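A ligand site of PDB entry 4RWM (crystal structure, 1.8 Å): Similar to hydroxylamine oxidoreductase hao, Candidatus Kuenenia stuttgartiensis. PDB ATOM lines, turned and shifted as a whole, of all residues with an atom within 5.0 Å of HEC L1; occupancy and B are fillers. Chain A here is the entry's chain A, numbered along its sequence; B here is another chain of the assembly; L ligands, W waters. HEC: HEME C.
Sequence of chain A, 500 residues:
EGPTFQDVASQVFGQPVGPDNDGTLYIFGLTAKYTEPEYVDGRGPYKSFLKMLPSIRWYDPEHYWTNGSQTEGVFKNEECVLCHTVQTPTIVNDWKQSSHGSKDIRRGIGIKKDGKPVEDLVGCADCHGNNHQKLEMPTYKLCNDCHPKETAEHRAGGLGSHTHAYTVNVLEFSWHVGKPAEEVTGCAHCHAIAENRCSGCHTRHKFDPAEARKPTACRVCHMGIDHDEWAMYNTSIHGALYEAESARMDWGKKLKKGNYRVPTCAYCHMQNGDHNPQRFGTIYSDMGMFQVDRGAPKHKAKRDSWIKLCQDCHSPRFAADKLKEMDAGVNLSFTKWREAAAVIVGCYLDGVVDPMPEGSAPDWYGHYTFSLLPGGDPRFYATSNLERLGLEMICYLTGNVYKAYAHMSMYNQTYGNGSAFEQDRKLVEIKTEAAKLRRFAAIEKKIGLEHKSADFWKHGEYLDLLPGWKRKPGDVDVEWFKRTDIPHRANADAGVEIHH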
ATOM      1  N   TRP A  58     -33.019 -24.120  -0.811  1.00  0.00           N
ATOM      2  CA  TRP A  58     -33.390 -25.342  -1.532  1.00  0.00           C
ATOM      3  C   TRP A  58     -34.726 -25.900  -1.054  1.00  0.00           C
ATOM      4  O   TRP A  58     -35.387 -26.627  -1.798  1.00  0.00           O
ATOM      5  CB  TRP A  58     -32.301 -26.406  -1.395  1.00  0.00           C
ATOM      6  CG  TRP A  58     -30.958 -25.935  -1.861  1.00  0.00           C
ATOM      7  CD1 TRP A  58     -29.968 -25.414  -1.083  1.00  0.00           C
ATOM      8  CD2 TRP A  58     -30.471 -25.916  -3.199  1.00  0.00           C
ATOM      9  NE1 TRP A  58     -28.887 -25.075  -1.856  1.00  0.00           N
ATOM     10  CE2 TRP A  58     -29.167 -25.377  -3.161  1.00  0.00           C
ATOM     11  CE3 TRP A  58     -30.994 -26.314  -4.438  1.00  0.00           C
ATOM     12  CZ2 TRP A  58     -28.395 -25.198  -4.307  1.00  0.00           C
ATOM     13  CZ3 TRP A  58     -30.223 -26.148  -5.578  1.00  0.00           C
ATOM     14  CH2 TRP A  58     -28.939 -25.595  -5.506  1.00  0.00           C
ATOM     15  N   TRP A  65     -35.258 -18.653  -2.667  1.00  0.00           N
ATOM     16  CA  TRP A  65     -34.475 -19.014  -3.856  1.00  0.00           C
ATOM     17  C   TRP A  65     -34.062 -17.775  -4.633  1.00  0.00           C
ATOM     18  O   TRP A  65     -34.880 -16.875  -4.874  1.00  0.00           O
ATOM     19  CB  TRP A  65     -35.245 -19.963  -4.777  1.00  0.00           C
ATOM     20  CG  TRP A  65     -34.449 -20.388  -5.972  1.00  0.00           C
ATOM     21  CD1 TRP A  65     -34.634 -19.968  -7.259  1.00  0.00           C
ATOM     22  CD2 TRP A  65     -33.330 -21.279  -5.987  1.00  0.00           C
ATOM     23  NE1 TRP A  65     -33.699 -20.568  -8.091  1.00  0.00           N
ATOM     24  CE2 TRP A  65     -32.885 -21.377  -7.328  1.00  0.00           C
ATOM     25  CE3 TRP A  65     -32.658 -22.009  -5.003  1.00  0.00           C
ATOM     26  CZ2 TRP A  65     -31.813 -22.175  -7.706  1.00  0.00           C
ATOM     27  CZ3 TRP A  65     -31.581 -22.800  -5.378  1.00  0.00           C
ATOM     28  CH2 TRP A  65     -31.168 -22.881  -6.717  1.00  0.00           C
ATOM     29  N   GLY A  68     -27.983 -18.202  -8.445  1.00  0.00           N
ATOM     30  CA  GLY A  68     -26.596 -18.319  -7.998  1.00  0.00           C
ATOM     31  C   GLY A  68     -25.737 -19.114  -8.960  1.00  0.00           C
ATOM     32  O   GLY A  68     -24.730 -19.706  -8.542  1.00  0.00           O
ATOM     33  N   SER A  69     -26.115 -19.117 -10.230  1.00  0.00           N
ATOM     34  CA  SER A  69     -25.388 -19.845 -11.269  1.00  0.00           C
ATOM     35  C   SER A  69     -24.388 -18.924 -11.973  1.00  0.00           C
ATOM     36  O   SER A  69     -24.598 -17.705 -12.047  1.00  0.00           O
ATOM     37  CB  SER A  69     -26.364 -20.416 -12.292  1.00  0.00           C
ATOM     38  OG  SER A  69     -25.689 -21.132 -13.319  1.00  0.00           O
ATOM     39  N   GLN A  70     -23.304 -19.513 -12.472  1.00  0.00           N
ATOM     40  CA  GLN A  70     -22.288 -18.782 -13.242  1.00  0.00           C
ATOM     41  C   GLN A  70     -22.445 -19.003 -14.757  1.00  0.00           C
ATOM     42  O   GLN A  70     -21.770 -18.361 -15.554  1.00  0.00           O
ATOM     43  CB  GLN A  70     -20.886 -19.187 -12.787  1.00  0.00           C
ATOM     44  CG  GLN A  70     -20.550 -18.784 -11.355  1.00  0.00           C
ATOM     45  CD  GLN A  70     -21.358 -19.545 -10.311  1.00  0.00           C
ATOM     46  OE1 GLN A  70     -21.981 -18.947  -9.435  1.00  0.00           O
ATOM     47  NE2 GLN A  70     -21.360 -20.876 -10.407  1.00  0.00           N
ATOM     48  N   THR A  71     -23.344 -19.905 -15.131  1.00  0.00           N
ATOM     49  CA  THR A  71     -23.553 -20.252 -16.544  1.00  0.00           C
ATOM     50  C   THR A  71     -24.663 -19.370 -17.111  1.00  0.00           C
ATOM     51  O   THR A  71     -25.728 -19.245 -16.511  1.00  0.00           O
ATOM     52  CB  THR A  71     -23.917 -21.741 -16.680  1.00  0.00           C
ATOM     53  OG1 THR A  71     -22.819 -22.540 -16.228  1.00  0.00           O
ATOM     54  CG2 THR A  71     -24.236 -22.115 -18.120  1.00  0.00           C
ATOM     55  N   PHE A  75     -31.570 -21.858 -23.199  1.00  0.00           N
ATOM     56  CA  PHE A  75     -31.312 -23.146 -23.831  1.00  0.00           C
ATOM     57  C   PHE A  75     -32.578 -23.969 -24.068  1.00  0.00           C
ATOM     58  O   PHE A  75     -33.571 -23.805 -23.360  1.00  0.00           O
ATOM     59  CB  PHE A  75     -30.358 -23.985 -22.963  1.00  0.00           C
ATOM     60  CG  PHE A  75     -29.023 -23.328 -22.720  1.00  0.00           C
ATOM     61  CD1 PHE A  75     -28.115 -23.156 -23.757  1.00  0.00           C
ATOM     62  CD2 PHE A  75     -28.665 -22.910 -21.448  1.00  0.00           C
ATOM     63  CE1 PHE A  75     -26.882 -22.556 -23.536  1.00  0.00           C
ATOM     64  CE2 PHE A  75     -27.427 -22.313 -21.219  1.00  0.00           C
ATOM     65  CZ  PHE A  75     -26.531 -22.134 -22.258  1.00  0.00           C
ATOM     66  N   LYS A  76     -32.507 -24.849 -25.057  1.00  0.00           N
ATOM     67  CA  LYS A  76     -33.565 -25.831 -25.329  1.00  0.00           C
ATOM     68  C   LYS A  76     -33.301 -27.055 -24.471  1.00  0.00           C
ATOM     69  O   LYS A  76     -32.159 -27.316 -24.088  1.00  0.00           O
ATOM     70  CB  LYS A  76     -33.551 -26.234 -26.804  1.00  0.00           C
ATOM     71  CG  LYS A  76     -33.661 -25.071 -27.791  1.00  0.00           C
ATOM     72  CD  LYS A  76     -33.420 -25.524 -29.224  1.00  0.00           C
ATOM     73  CE  LYS A  76     -33.515 -24.348 -30.199  1.00  0.00           C
ATOM     74  NZ  LYS A  76     -33.317 -24.771 -31.616  1.00  0.00           N
ATOM     75  N   GLU A  79     -30.298 -29.185 -25.152  1.00  0.00           N
ATOM     76  CA  GLU A  79     -29.033 -28.548 -24.773  1.00  0.00           C
ATOM     77  C   GLU A  79     -28.751 -28.702 -23.276  1.00  0.00           C
ATOM     78  O   GLU A  79     -27.601 -28.952 -22.905  1.00  0.00           O
ATOM     79  CB  GLU A  79     -29.045 -27.078 -25.201  1.00  0.00           C
ATOM     80  CG  GLU A  79     -29.113 -26.927 -26.727  1.00  0.00           C
ATOM     81  CD  GLU A  79     -29.315 -25.504 -27.210  1.00  0.00           C
ATOM     82  OE1 GLU A  79     -28.875 -25.212 -28.338  1.00  0.00           O
ATOM     83  OE2 GLU A  79     -29.925 -24.688 -26.491  1.00  0.00           O
ATOM     84  N   CYS A  80     -29.779 -28.585 -22.443  1.00  0.00           N
ATOM     85  CA  CYS A  80     -29.655 -28.905 -21.009  1.00  0.00           C
ATOM     86  C   CYS A  80     -29.019 -30.285 -20.829  1.00  0.00           C
ATOM     87  O   CYS A  80     -28.061 -30.449 -20.071  1.00  0.00           O
ATOM     88  CB  CYS A  80     -31.015 -28.929 -20.302  1.00  0.00           C
ATOM     89  SG  CYS A  80     -32.126 -27.543 -20.567  1.00  0.00           S
ATOM     90  N   CYS A  83     -25.101 -30.785 -22.084  1.00  0.00           N
ATOM     91  CA  CYS A  83     -24.087 -30.224 -21.193  1.00  0.00           C
ATOM     92  C   CYS A  83     -24.069 -30.922 -19.833  1.00  0.00           C
ATOM     93  O   CYS A  83     -23.000 -31.218 -19.296  1.00  0.00           O
ATOM     94  CB  CYS A  83     -24.298 -28.730 -21.018  1.00  0.00           C
ATOM     95  SG  CYS A  83     -22.936 -27.925 -20.172  1.00  0.00           S
ATOM     96  N   HIS A  84     -25.248 -31.167 -19.272  1.00  0.00           N
ATOM     97  CA  HIS A  84     -25.330 -31.824 -17.957  1.00  0.00           C
ATOM     98  C   HIS A  84     -24.941 -33.299 -17.982  1.00  0.00           C
ATOM     99  O   HIS A  84     -24.644 -33.882 -16.934  1.00  0.00           O
ATOM    100  CB  HIS A  84     -26.713 -31.612 -17.311  1.00  0.00           C
ATOM    101  CG  HIS A  84     -26.845 -30.289 -16.617  1.00  0.00           C
ATOM    102  ND1 HIS A  84     -26.547 -30.121 -15.283  1.00  0.00           N
ATOM    103  CD2 HIS A  84     -27.185 -29.063 -17.090  1.00  0.00           C
ATOM    104  CE1 HIS A  84     -26.710 -28.853 -14.954  1.00  0.00           C
ATOM    105  NE2 HIS A  84     -27.098 -28.191 -16.033  1.00  0.00           N
ATOM    106  N   GLN A  87     -21.593 -32.394 -17.021  1.00  0.00           N
ATOM    107  CA  GLN A  87     -21.448 -31.583 -15.799  1.00  0.00           C
ATOM    108  C   GLN A  87     -22.082 -32.168 -14.526  1.00  0.00           C
ATOM    109  O   GLN A  87     -21.554 -31.969 -13.430  1.00  0.00           O
ATOM    110  CB  GLN A  87     -21.937 -30.161 -16.043  1.00  0.00           C
ATOM    111  CG  GLN A  87     -20.994 -29.339 -16.926  1.00  0.00           C
ATOM    112  CD  GLN A  87     -19.645 -29.139 -16.275  1.00  0.00           C
ATOM    113  OE1 GLN A  87     -19.549 -28.964 -15.049  1.00  0.00           O
ATOM    114  NE2 GLN A  87     -18.583 -29.176 -17.083  1.00  0.00           N
ATOM    115  N   CYS A 124     -35.474 -30.944 -18.596  1.00  0.00           N
ATOM    116  CA  CYS A 124     -34.908 -30.081 -17.547  1.00  0.00           C
ATOM    117  C   CYS A 124     -35.549 -28.696 -17.552  1.00  0.00           C
ATOM    118  O   CYS A 124     -35.869 -28.155 -16.488  1.00  0.00           O
ATOM    119  CB  CYS A 124     -33.385 -29.916 -17.726  1.00  0.00           C
ATOM    120  SG  CYS A 124     -32.456 -31.400 -18.213  1.00  0.00           S
ATOM    121  N   ALA A 125     -35.721 -28.131 -18.751  1.00  0.00           N
ATOM    122  CA  ALA A 125     -36.232 -26.768 -18.899  1.00  0.00           C
ATOM    123  C   ALA A 125     -37.710 -26.651 -18.549  1.00  0.00           C
ATOM    124  O   ALA A 125     -38.173 -25.600 -18.109  1.00  0.00           O
ATOM    125  CB  ALA A 125     -35.978 -26.236 -20.311  1.00  0.00           C
ATOM    126  N   HIS A 128     -37.307 -26.519 -14.695  1.00  0.00           N
ATOM    127  CA  HIS A 128     -36.374 -25.550 -14.108  1.00  0.00           C
ATOM    128  C   HIS A 128     -36.322 -24.200 -14.838  1.00  0.00           C
ATOM    129  O   HIS A 128     -35.702 -23.260 -14.351  1.00  0.00           O
ATOM    130  CB  HIS A 128     -34.969 -26.147 -14.051  1.00  0.00           C
ATOM    131  CG  HIS A 128     -34.844 -27.289 -13.087  1.00  0.00           C
ATOM    132  ND1 HIS A 128     -34.912 -27.109 -11.720  1.00  0.00           N
ATOM    133  CD2 HIS A 128     -34.634 -28.615 -13.283  1.00  0.00           C
ATOM    134  CE1 HIS A 128     -34.768 -28.274 -11.120  1.00  0.00           C
ATOM    135  NE2 HIS A 128     -34.599 -29.211 -12.044  1.00  0.00           N
ATOM    136  N   GLY A 129     -36.959 -24.116 -16.005  1.00  0.00           N
ATOM    137  CA  GLY A 129     -36.885 -22.912 -16.846  1.00  0.00           C
ATOM    138  C   GLY A 129     -35.780 -22.984 -17.882  1.00  0.00           C
ATOM    139  O   GLY A 129     -34.895 -23.840 -17.775  1.00  0.00           O
ATOM    140  N   ASN A 130     -35.829 -22.094 -18.879  1.00  0.00           N
ATOM    141  CA  ASN A 130     -34.905 -22.123 -20.028  1.00  0.00           C
ATOM    142  C   ASN A 130     -33.698 -21.197 -19.892  1.00  0.00           C
ATOM    143  O   ASN A 130     -32.700 -21.379 -20.587  1.00  0.00           O
ATOM    144  CB  ASN A 130     -35.633 -21.738 -21.320  1.00  0.00           C
ATOM    145  CG  ASN A 130     -36.727 -22.697 -21.699  1.00  0.00           C
ATOM    146  OD1 ASN A 130     -37.888 -22.529 -21.303  1.00  0.00           O
ATOM    147  ND2 ASN A 130     -36.377 -23.716 -22.494  1.00  0.00           N
ATOM    148  N   HIS A 132     -30.594 -19.828 -17.905  1.00  0.00           N
ATOM    149  CA  HIS A 132     -29.702 -20.362 -16.877  1.00  0.00           C
ATOM    150  C   HIS A 132     -29.368 -19.344 -15.768  1.00  0.00           C
ATOM    151  O   HIS A 132     -28.798 -19.708 -14.734  1.00  0.00           O
ATOM    152  CB  HIS A 132     -28.415 -20.924 -17.497  1.00  0.00           C
ATOM    153  CG  HIS A 132     -27.902 -22.150 -16.790  1.00  0.00           C
ATOM    154  ND1 HIS A 132     -27.229 -22.089 -15.588  1.00  0.00           N
ATOM    155  CD2 HIS A 132     -27.994 -23.460 -17.106  1.00  0.00           C
ATOM    156  CE1 HIS A 132     -26.930 -23.319 -15.197  1.00  0.00           C
ATOM    157  NE2 HIS A 132     -27.373 -24.164 -16.115  1.00  0.00           N
ATOM    158  N   LEU A 135     -33.012 -19.734 -13.250  1.00  0.00           N
ATOM    159  CA  LEU A 135     -33.449 -21.104 -13.013  1.00  0.00           C
ATOM    160  C   LEU A 135     -34.363 -21.175 -11.810  1.00  0.00           C
ATOM    161  O   LEU A 135     -34.236 -20.389 -10.865  1.00  0.00           O
ATOM    162  CB  LEU A 135     -32.252 -22.053 -12.823  1.00  0.00           C
ATOM    163  CG  LEU A 135     -31.365 -22.252 -14.047  1.00  0.00           C
ATOM    164  CD1 LEU A 135     -30.059 -22.941 -13.645  1.00  0.00           C
ATOM    165  CD2 LEU A 135     -32.076 -23.037 -15.145  1.00  0.00           C
ATOM    166  N   MET A 137     -36.279 -23.455  -8.738  1.00  0.00           N
ATOM    167  CA  MET A 137     -36.149 -24.592  -7.852  1.00  0.00           C
ATOM    168  C   MET A 137     -37.560 -24.911  -7.336  1.00  0.00           C
ATOM    169  O   MET A 137     -38.107 -24.164  -6.525  1.00  0.00           O
ATOM    170  CB  MET A 137     -35.179 -24.266  -6.718  1.00  0.00           C
ATOM    171  CG  MET A 137     -34.579 -25.455  -6.017  1.00  0.00           C
ATOM    172  SD  MET A 137     -33.915 -26.754  -7.097  1.00  0.00           S
ATOM    173  CE  MET A 137     -32.845 -25.881  -8.223  1.00  0.00           C
ATOM    174  N   GLN B 311     -20.543 -33.149  -7.337  1.00  0.00           N
ATOM    175  CA  GLN B 311     -21.075 -32.687  -8.613  1.00  0.00           C
ATOM    176  C   GLN B 311     -21.198 -33.809  -9.661  1.00  0.00           C
ATOM    177  O   GLN B 311     -21.795 -33.612 -10.709  1.00  0.00           O
ATOM    178  CB  GLN B 311     -20.244 -31.525  -9.180  1.00  0.00           C
ATOM    179  CG  GLN B 311     -20.948 -30.717 -10.270  1.00  0.00           C
ATOM    180  CD  GLN B 311     -20.064 -29.649 -10.898  1.00  0.00           C
ATOM    181  OE1 GLN B 311     -19.205 -29.067 -10.226  1.00  0.00           O
ATOM    182  NE2 GLN B 311     -20.275 -29.389 -12.184  1.00  0.00           N
ATOM    183  N   SER B 315     -25.832 -30.291  -8.290  1.00  0.00           N
ATOM    184  CA  SER B 315     -25.338 -28.928  -8.435  1.00  0.00           C
ATOM    185  C   SER B 315     -24.190 -28.671  -7.448  1.00  0.00           C
ATOM    186  O   SER B 315     -24.275 -29.079  -6.289  1.00  0.00           O
ATOM    187  CB  SER B 315     -26.455 -27.937  -8.129  1.00  0.00           C
ATOM    188  OG  SER B 315     -25.931 -26.681  -7.728  1.00  0.00           O
ATOM    189  N   PRO B 316     -23.115 -28.004  -7.901  1.00  0.00           N
ATOM    190  CA  PRO B 316     -22.024 -27.689  -6.976  1.00  0.00           C
ATOM    191  C   PRO B 316     -22.412 -26.633  -5.929  1.00  0.00           C
ATOM    192  O   PRO B 316     -21.773 -26.564  -4.871  1.00  0.00           O
ATOM    193  CB  PRO B 316     -20.930 -27.146  -7.901  1.00  0.00           C
ATOM    194  CG  PRO B 316     -21.663 -26.575  -9.044  1.00  0.00           C
ATOM    195  CD  PRO B 316     -22.858 -27.467  -9.246  1.00  0.00           C
ATOM    196  N   ARG B 317     -23.417 -25.818  -6.220  1.00  0.00           N
ATOM    197  CA  ARG B 317     -23.952 -24.857  -5.269  1.00  0.00           C
ATOM    198  C   ARG B 317     -24.643 -25.589  -4.123  1.00  0.00           C
ATOM    199  O   ARG B 317     -24.436 -25.273  -2.949  1.00  0.00           O
ATOM    200  CB  ARG B 317     -24.936 -23.929  -5.964  1.00  0.00           C
ATOM    201  CG  ARG B 317     -25.430 -22.750  -5.134  1.00  0.00           C
ATOM    202  CD  ARG B 317     -26.564 -22.049  -5.855  1.00  0.00           C
ATOM    203  NE  ARG B 317     -27.040 -20.858  -5.159  1.00  0.00           N
ATOM    204  CZ  ARG B 317     -28.145 -20.187  -5.499  1.00  0.00           C
ATOM    205  NH1 ARG B 317     -28.894 -20.575  -6.529  1.00  0.00           N
ATOM    206  NH2 ARG B 317     -28.481 -19.107  -4.795  1.00  0.00           N
ATOM    207  N   PHE B 318     -25.461 -26.573  -4.476  1.00  0.00           N
ATOM    208  CA  PHE B 318     -26.101 -27.455  -3.486  1.00  0.00           C
ATOM    209  C   PHE B 318     -25.059 -28.148  -2.601  1.00  0.00           C
ATOM    210  O   PHE B 318     -25.159 -28.102  -1.369  1.00  0.00           O
ATOM    211  CB  PHE B 318     -26.978 -28.496  -4.188  1.00  0.00           C
ATOM    212  CG  PHE B 318     -27.653 -29.452  -3.245  1.00  0.00           C
ATOM    213  CD1 PHE B 318     -28.588 -29.002  -2.317  1.00  0.00           C
ATOM    214  CD2 PHE B 318     -27.342 -30.804  -3.270  1.00  0.00           C
ATOM    215  CE1 PHE B 318     -29.202 -29.881  -1.445  1.00  0.00           C
ATOM    216  CE2 PHE B 318     -27.956 -31.696  -2.392  1.00  0.00           C
ATOM    217  CZ  PHE B 318     -28.888 -31.231  -1.484  1.00  0.00           C
HETATM  218 FE   HEC L   1     -27.237 -26.184 -16.115  1.00  0.00          FE
HETATM  219  CHA HEC L   1     -26.206 -25.736 -12.865  1.00  0.00           C
HETATM  220  CHB HEC L   1     -30.421 -26.739 -15.024  1.00  0.00           C
HETATM  221  CHC HEC L   1     -28.352 -25.979 -19.344  1.00  0.00           C
HETATM  222  CHD HEC L   1     -24.003 -26.235 -17.206  1.00  0.00           C
HETATM  223  NA  HEC L   1     -28.143 -26.246 -14.274  1.00  0.00           N
HETATM  224  C1A HEC L   1     -27.545 -25.984 -13.068  1.00  0.00           C
HETATM  225  C2A HEC L   1     -28.565 -26.011 -12.049  1.00  0.00           C
HETATM  226  C3A HEC L   1     -29.731 -26.289 -12.634  1.00  0.00           C
HETATM  227  C4A HEC L   1     -29.487 -26.445 -14.055  1.00  0.00           C
HETATM  228  CMA HEC L   1     -31.107 -26.417 -11.938  1.00  0.00           C
HETATM  229  CAA HEC L   1     -28.298 -25.714 -10.558  1.00  0.00           C
HETATM  230  CBA HEC L   1     -28.313 -24.188 -10.417  1.00  0.00           C
HETATM  231  CGA HEC L   1     -27.892 -23.708  -9.058  1.00  0.00           C
HETATM  232  O1A HEC L   1     -27.045 -24.381  -8.394  1.00  0.00           O
HETATM  233  O2A HEC L   1     -28.409 -22.650  -8.621  1.00  0.00           O
HETATM  234  NB  HEC L   1     -29.035 -26.372 -17.020  1.00  0.00           N
HETATM  235  C1B HEC L   1     -30.249 -26.527 -16.374  1.00  0.00           C
HETATM  236  C2B HEC L   1     -31.299 -26.420 -17.356  1.00  0.00           C
HETATM  237  C3B HEC L   1     -30.727 -26.216 -18.548  1.00  0.00           C
HETATM  238  C4B HEC L   1     -29.295 -26.186 -18.370  1.00  0.00           C
HETATM  239  CMB HEC L   1     -32.813 -26.526 -17.058  1.00  0.00           C
HETATM  240  CAB HEC L   1     -31.469 -26.024 -19.876  1.00  0.00           C
HETATM  241  CBB HEC L   1     -32.338 -25.007 -19.965  1.00  0.00           C
HETATM  242  NC  HEC L   1     -26.338 -26.113 -17.934  1.00  0.00           N
HETATM  243  C1C HEC L   1     -26.986 -26.033 -19.149  1.00  0.00           C
HETATM  244  C2C HEC L   1     -25.977 -26.030 -20.188  1.00  0.00           C
HETATM  245  C3C HEC L   1     -24.765 -26.102 -19.597  1.00  0.00           C
HETATM  246  C4C HEC L   1     -24.982 -26.159 -18.170  1.00  0.00           C
HETATM  247  CMC HEC L   1     -26.308 -25.964 -21.694  1.00  0.00           C
HETATM  248  CAC HEC L   1     -23.368 -26.164 -20.271  1.00  0.00           C
HETATM  249  CBC HEC L   1     -23.184 -25.718 -21.520  1.00  0.00           C
HETATM  250  ND  HEC L   1     -25.413 -26.003 -15.191  1.00  0.00           N
HETATM  251  C1D HEC L   1     -24.188 -26.080 -15.860  1.00  0.00           C
HETATM  252  C2D HEC L   1     -23.117 -25.950 -14.899  1.00  0.00           C
HETATM  253  C3D HEC L   1     -23.789 -25.790 -13.554  1.00  0.00           C
HETATM  254  C4D HEC L   1     -25.215 -25.847 -13.829  1.00  0.00           C
HETATM  255  CMD HEC L   1     -21.591 -25.962 -15.166  1.00  0.00           C
HETATM  256  CAD HEC L   1     -23.103 -25.625 -12.196  1.00  0.00           C
HETATM  257  CBD HEC L   1     -22.326 -24.310 -12.149  1.00  0.00           C
HETATM  258  CGD HEC L   1     -23.199 -23.131 -12.509  1.00  0.00           C
HETATM  259  O1D HEC L   1     -22.745 -22.313 -13.357  1.00  0.00           O
HETATM  260  O2D HEC L   1     -24.327 -23.016 -11.967  1.00  0.00           O
HETATM  261 FE   HEC L   2     -34.195 -31.145 -11.611  1.00  0.00          FE
HETATM  262  CHA HEC L   2     -33.519 -30.279  -8.350  1.00  0.00           C
HETATM  263  CHB HEC L   2     -31.046 -30.309 -12.547  1.00  0.00           C
HETATM  264  CHC HEC L   2     -34.797 -32.475 -14.701  1.00  0.00           C
HETATM  265  CHD HEC L   2     -37.555 -31.408 -10.897  1.00  0.00           C
HETATM  266  NA  HEC L   2     -32.577 -30.443 -10.616  1.00  0.00           N
HETATM  267  C1A HEC L   2     -32.491 -30.142  -9.272  1.00  0.00           C
HETATM  268  C2A HEC L   2     -31.147 -29.681  -9.003  1.00  0.00           C
HETATM  269  C3A HEC L   2     -30.461 -29.698 -10.158  1.00  0.00           C
HETATM  270  C4A HEC L   2     -31.354 -30.169 -11.200  1.00  0.00           C
HETATM  271  CMA HEC L   2     -28.986 -29.280 -10.370  1.00  0.00           C
HETATM  272  CAA HEC L   2     -30.614 -29.244  -7.619  1.00  0.00           C
HETATM  273  CBA HEC L   2     -30.592 -30.380  -6.603  1.00  0.00           C
HETATM  274  CGA HEC L   2     -29.373 -31.248  -6.783  1.00  0.00           C
HETATM  275  O1A HEC L   2     -29.496 -32.487  -6.571  1.00  0.00           O
HETATM  276  O2A HEC L   2     -28.294 -30.705  -7.114  1.00  0.00           O
HETATM  277  NB  HEC L   2     -33.129 -31.330 -13.314  1.00  0.00           N
HETATM  278  C1B HEC L   2     -31.820 -30.937 -13.491  1.00  0.00           C
HETATM  279  C2B HEC L   2     -31.417 -31.313 -14.836  1.00  0.00           C
HETATM  280  C3B HEC L   2     -32.456 -31.916 -15.410  1.00  0.00           C
HETATM  281  C4B HEC L   2     -33.553 -31.940 -14.472  1.00  0.00           C
HETATM  282  CMB HEC L   2     -30.022 -31.049 -15.465  1.00  0.00           C
HETATM  283  CAB HEC L   2     -32.517 -32.519 -16.811  1.00  0.00           C
HETATM  284  CBB HEC L   2     -31.682 -33.548 -17.059  1.00  0.00           C
HETATM  285  NC  HEC L   2     -35.870 -31.855 -12.591  1.00  0.00           N
HETATM  286  C1C HEC L   2     -35.896 -32.263 -13.914  1.00  0.00           C
HETATM  287  C2C HEC L   2     -37.278 -32.416 -14.310  1.00  0.00           C
HETATM  288  C3C HEC L   2     -38.051 -32.116 -13.266  1.00  0.00           C
HETATM  289  C4C HEC L   2     -37.173 -31.758 -12.162  1.00  0.00           C
HETATM  290  CMC HEC L   2     -37.740 -32.849 -15.723  1.00  0.00           C
HETATM  291  CAC HEC L   2     -39.601 -32.108 -13.260  1.00  0.00           C
HETATM  292  CBC HEC L   2     -40.258 -33.240 -13.548  1.00  0.00           C
HETATM  293  ND  HEC L   2     -35.331 -30.930  -9.876  1.00  0.00           N
HETATM  294  C1D HEC L   2     -36.723 -31.031  -9.858  1.00  0.00           C
HETATM  295  C2D HEC L   2     -37.205 -30.673  -8.555  1.00  0.00           C
HETATM  296  C3D HEC L   2     -35.960 -30.317  -7.752  1.00  0.00           C
HETATM  297  C4D HEC L   2     -34.838 -30.501  -8.654  1.00  0.00           C
HETATM  298  CMD HEC L   2     -38.660 -30.640  -8.058  1.00  0.00           C
HETATM  299  CAD HEC L   2     -35.938 -29.825  -6.287  1.00  0.00           C
HETATM  300  CBD HEC L   2     -35.459 -30.889  -5.324  1.00  0.00           C
HETATM  301  CGD HEC L   2     -36.528 -31.902  -5.034  1.00  0.00           C
HETATM  302  O1D HEC L   2     -36.158 -33.075  -4.744  1.00  0.00           O
HETATM  303  O2D HEC L   2     -37.743 -31.559  -5.078  1.00  0.00           O
HETATM  304  O   HOH W   1     -24.582 -24.063  -9.561  1.00  0.00           O
HETATM  305  O   HOH W   2     -18.448 -26.144 -15.770  1.00  0.00           O
HETATM  306  O   HOH W   3     -29.247 -20.405  -9.797  1.00  0.00           O
HETATM  307  O   HOH W   4     -20.145 -22.431 -14.089  1.00  0.00           O
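A ring nitrogen (ND1) of His 132 is in hydrogen-bond range of the side-chain hydroxyl (OG) of Ser 69 (2.9 Å).
The backbone carbonyl oxygen of Thr 71 lies close to a ring nitrogen (ND1) of His 132 (3.3 Å).
The side-chain hydroxyl (OG) of Ser 315 of chain B lies within hydrogen-bond range of the backbone NH (N) of Phe 318 of chain B (3.3 Å).
N of Thr 71 is in hydrogen-bond range of OG of Ser 69 (3.2 Å).
The side-chain amide oxygen of Gln 70 sits close to the backbone carbonyl oxygen of Gly 68, at 3.0 Å.
The backbone carbonyl oxygen (O) of Leu 135 lies within hydrogen-bond range of the indole nitrogen (NE1) of Trp 65 (2.8 Å).
NE2 of Gln 311 of chain B lies within hydrogen-bond range of OE1 of Gln 87 (3.0 Å).
N of Phe 75 lies within hydrogen-bond range of O of Asn 130, 2.9 Å away.
Water W1 lies within hydrogen-bond range of O2D of HEC L1 (2.6 Å) and OG of Ser 315 of chain B (3.5 Å).
Water W4 bridges O1D of HEC L1 (2.7 Å) and OG1 of Thr 71 (3.4 Å).
Trp 58 touches HEC L1 (CH2 to O1A, 3.7 Å).
Trp 65 touches HEC L1.
Phe 75 touches HEC L1 (CD2 to CHC, 3.7 Å).
O of Glu 79 touches CMC of HEC L1 (3.5 Å).
Gln 87 touches HEC L1 (OE1 to CMD, 3.6 Å).
Cys 124 touches HEC L1 (CB to CMB, 3.5 Å).
N of Ala 125 touches CMB of HEC L1, at 3.7 Å.
His 128 touches HEC L1.
O of Gly 129 touches CMB of HEC L1 (3.5 Å).
O of Asn 130 touches CBB of HEC L1, at 3.7 Å.
Leu 135 touches HEC L1 (CD1 to C3A, 3.5 Å).
Pro 316 of chain B touches HEC L1 (CD to CAD, 3.5 Å).
Hydrophobic or aromatic side chains that line HEC L1: Trp 58, Trp 65, Phe 75, His 84, Ala 125, His 128, His 132, Leu 135 and Pro 316 of chain B.
Within 4 Å of HEC L1: Trp 58, Trp 65, Ser 69, Gln 70, Thr 71, Phe 75, Glu 79, Cys 80, Cys 83, His 84, Gln 87, Cys 124, Ala 125, His 128, Gly 129, Asn 130, His 132, Leu 135, Ser 315 of chain B, Pro 316 of chain B and Arg 317 of chain B.
The nearest printed residue that does not touch HEC L1 is Met 137 (4.1 Å).
The side-chain sulfur (SG) of Cys 80 is bonded to a carbon (CAB) of HEC L1 (1.8 Å).
A carbon (CAC) of HEC L1 is covalently linked to the side-chain sulfur (SG) of Cys 83.
NE2 of His 84 binds FE of HEC L1.
FE of HEC L1 is bound by NE2 of His 132.
OG of Ser 315 of chain B lies within hydrogen-bond range of O1A of HEC L1.
O2D of HEC L1 lies within hydrogen-bond range of OG of Ser 69 (2.7 Å).
N of Thr 71 lies within hydrogen-bond range of O1D of HEC L1 (3.1 Å).
An oxygen (O1D) of HEC L1 lies within hydrogen-bond range of the side-chain hydroxyl of Thr 71.
The guanidinium group of Arg 317 of chain B is in salt-bridge range of an oxygen (O2A) of HEC L1.
The backbone NH (N) of Gln 70 is in hydrogen-bond range of an oxygen (O1D) of HEC L1, 3.0 Å away.
N of Ser 315 of chain B lies within hydrogen-bond range of O2A of HEC L2 (2.8 Å).
SG of Cys 124 is covalently linked to CAB of HEC L2 (1.8 Å).
A ring nitrogen (NE2) of His 128 binds an iron atom (FE) of HEC L2, 2.0 Å away.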
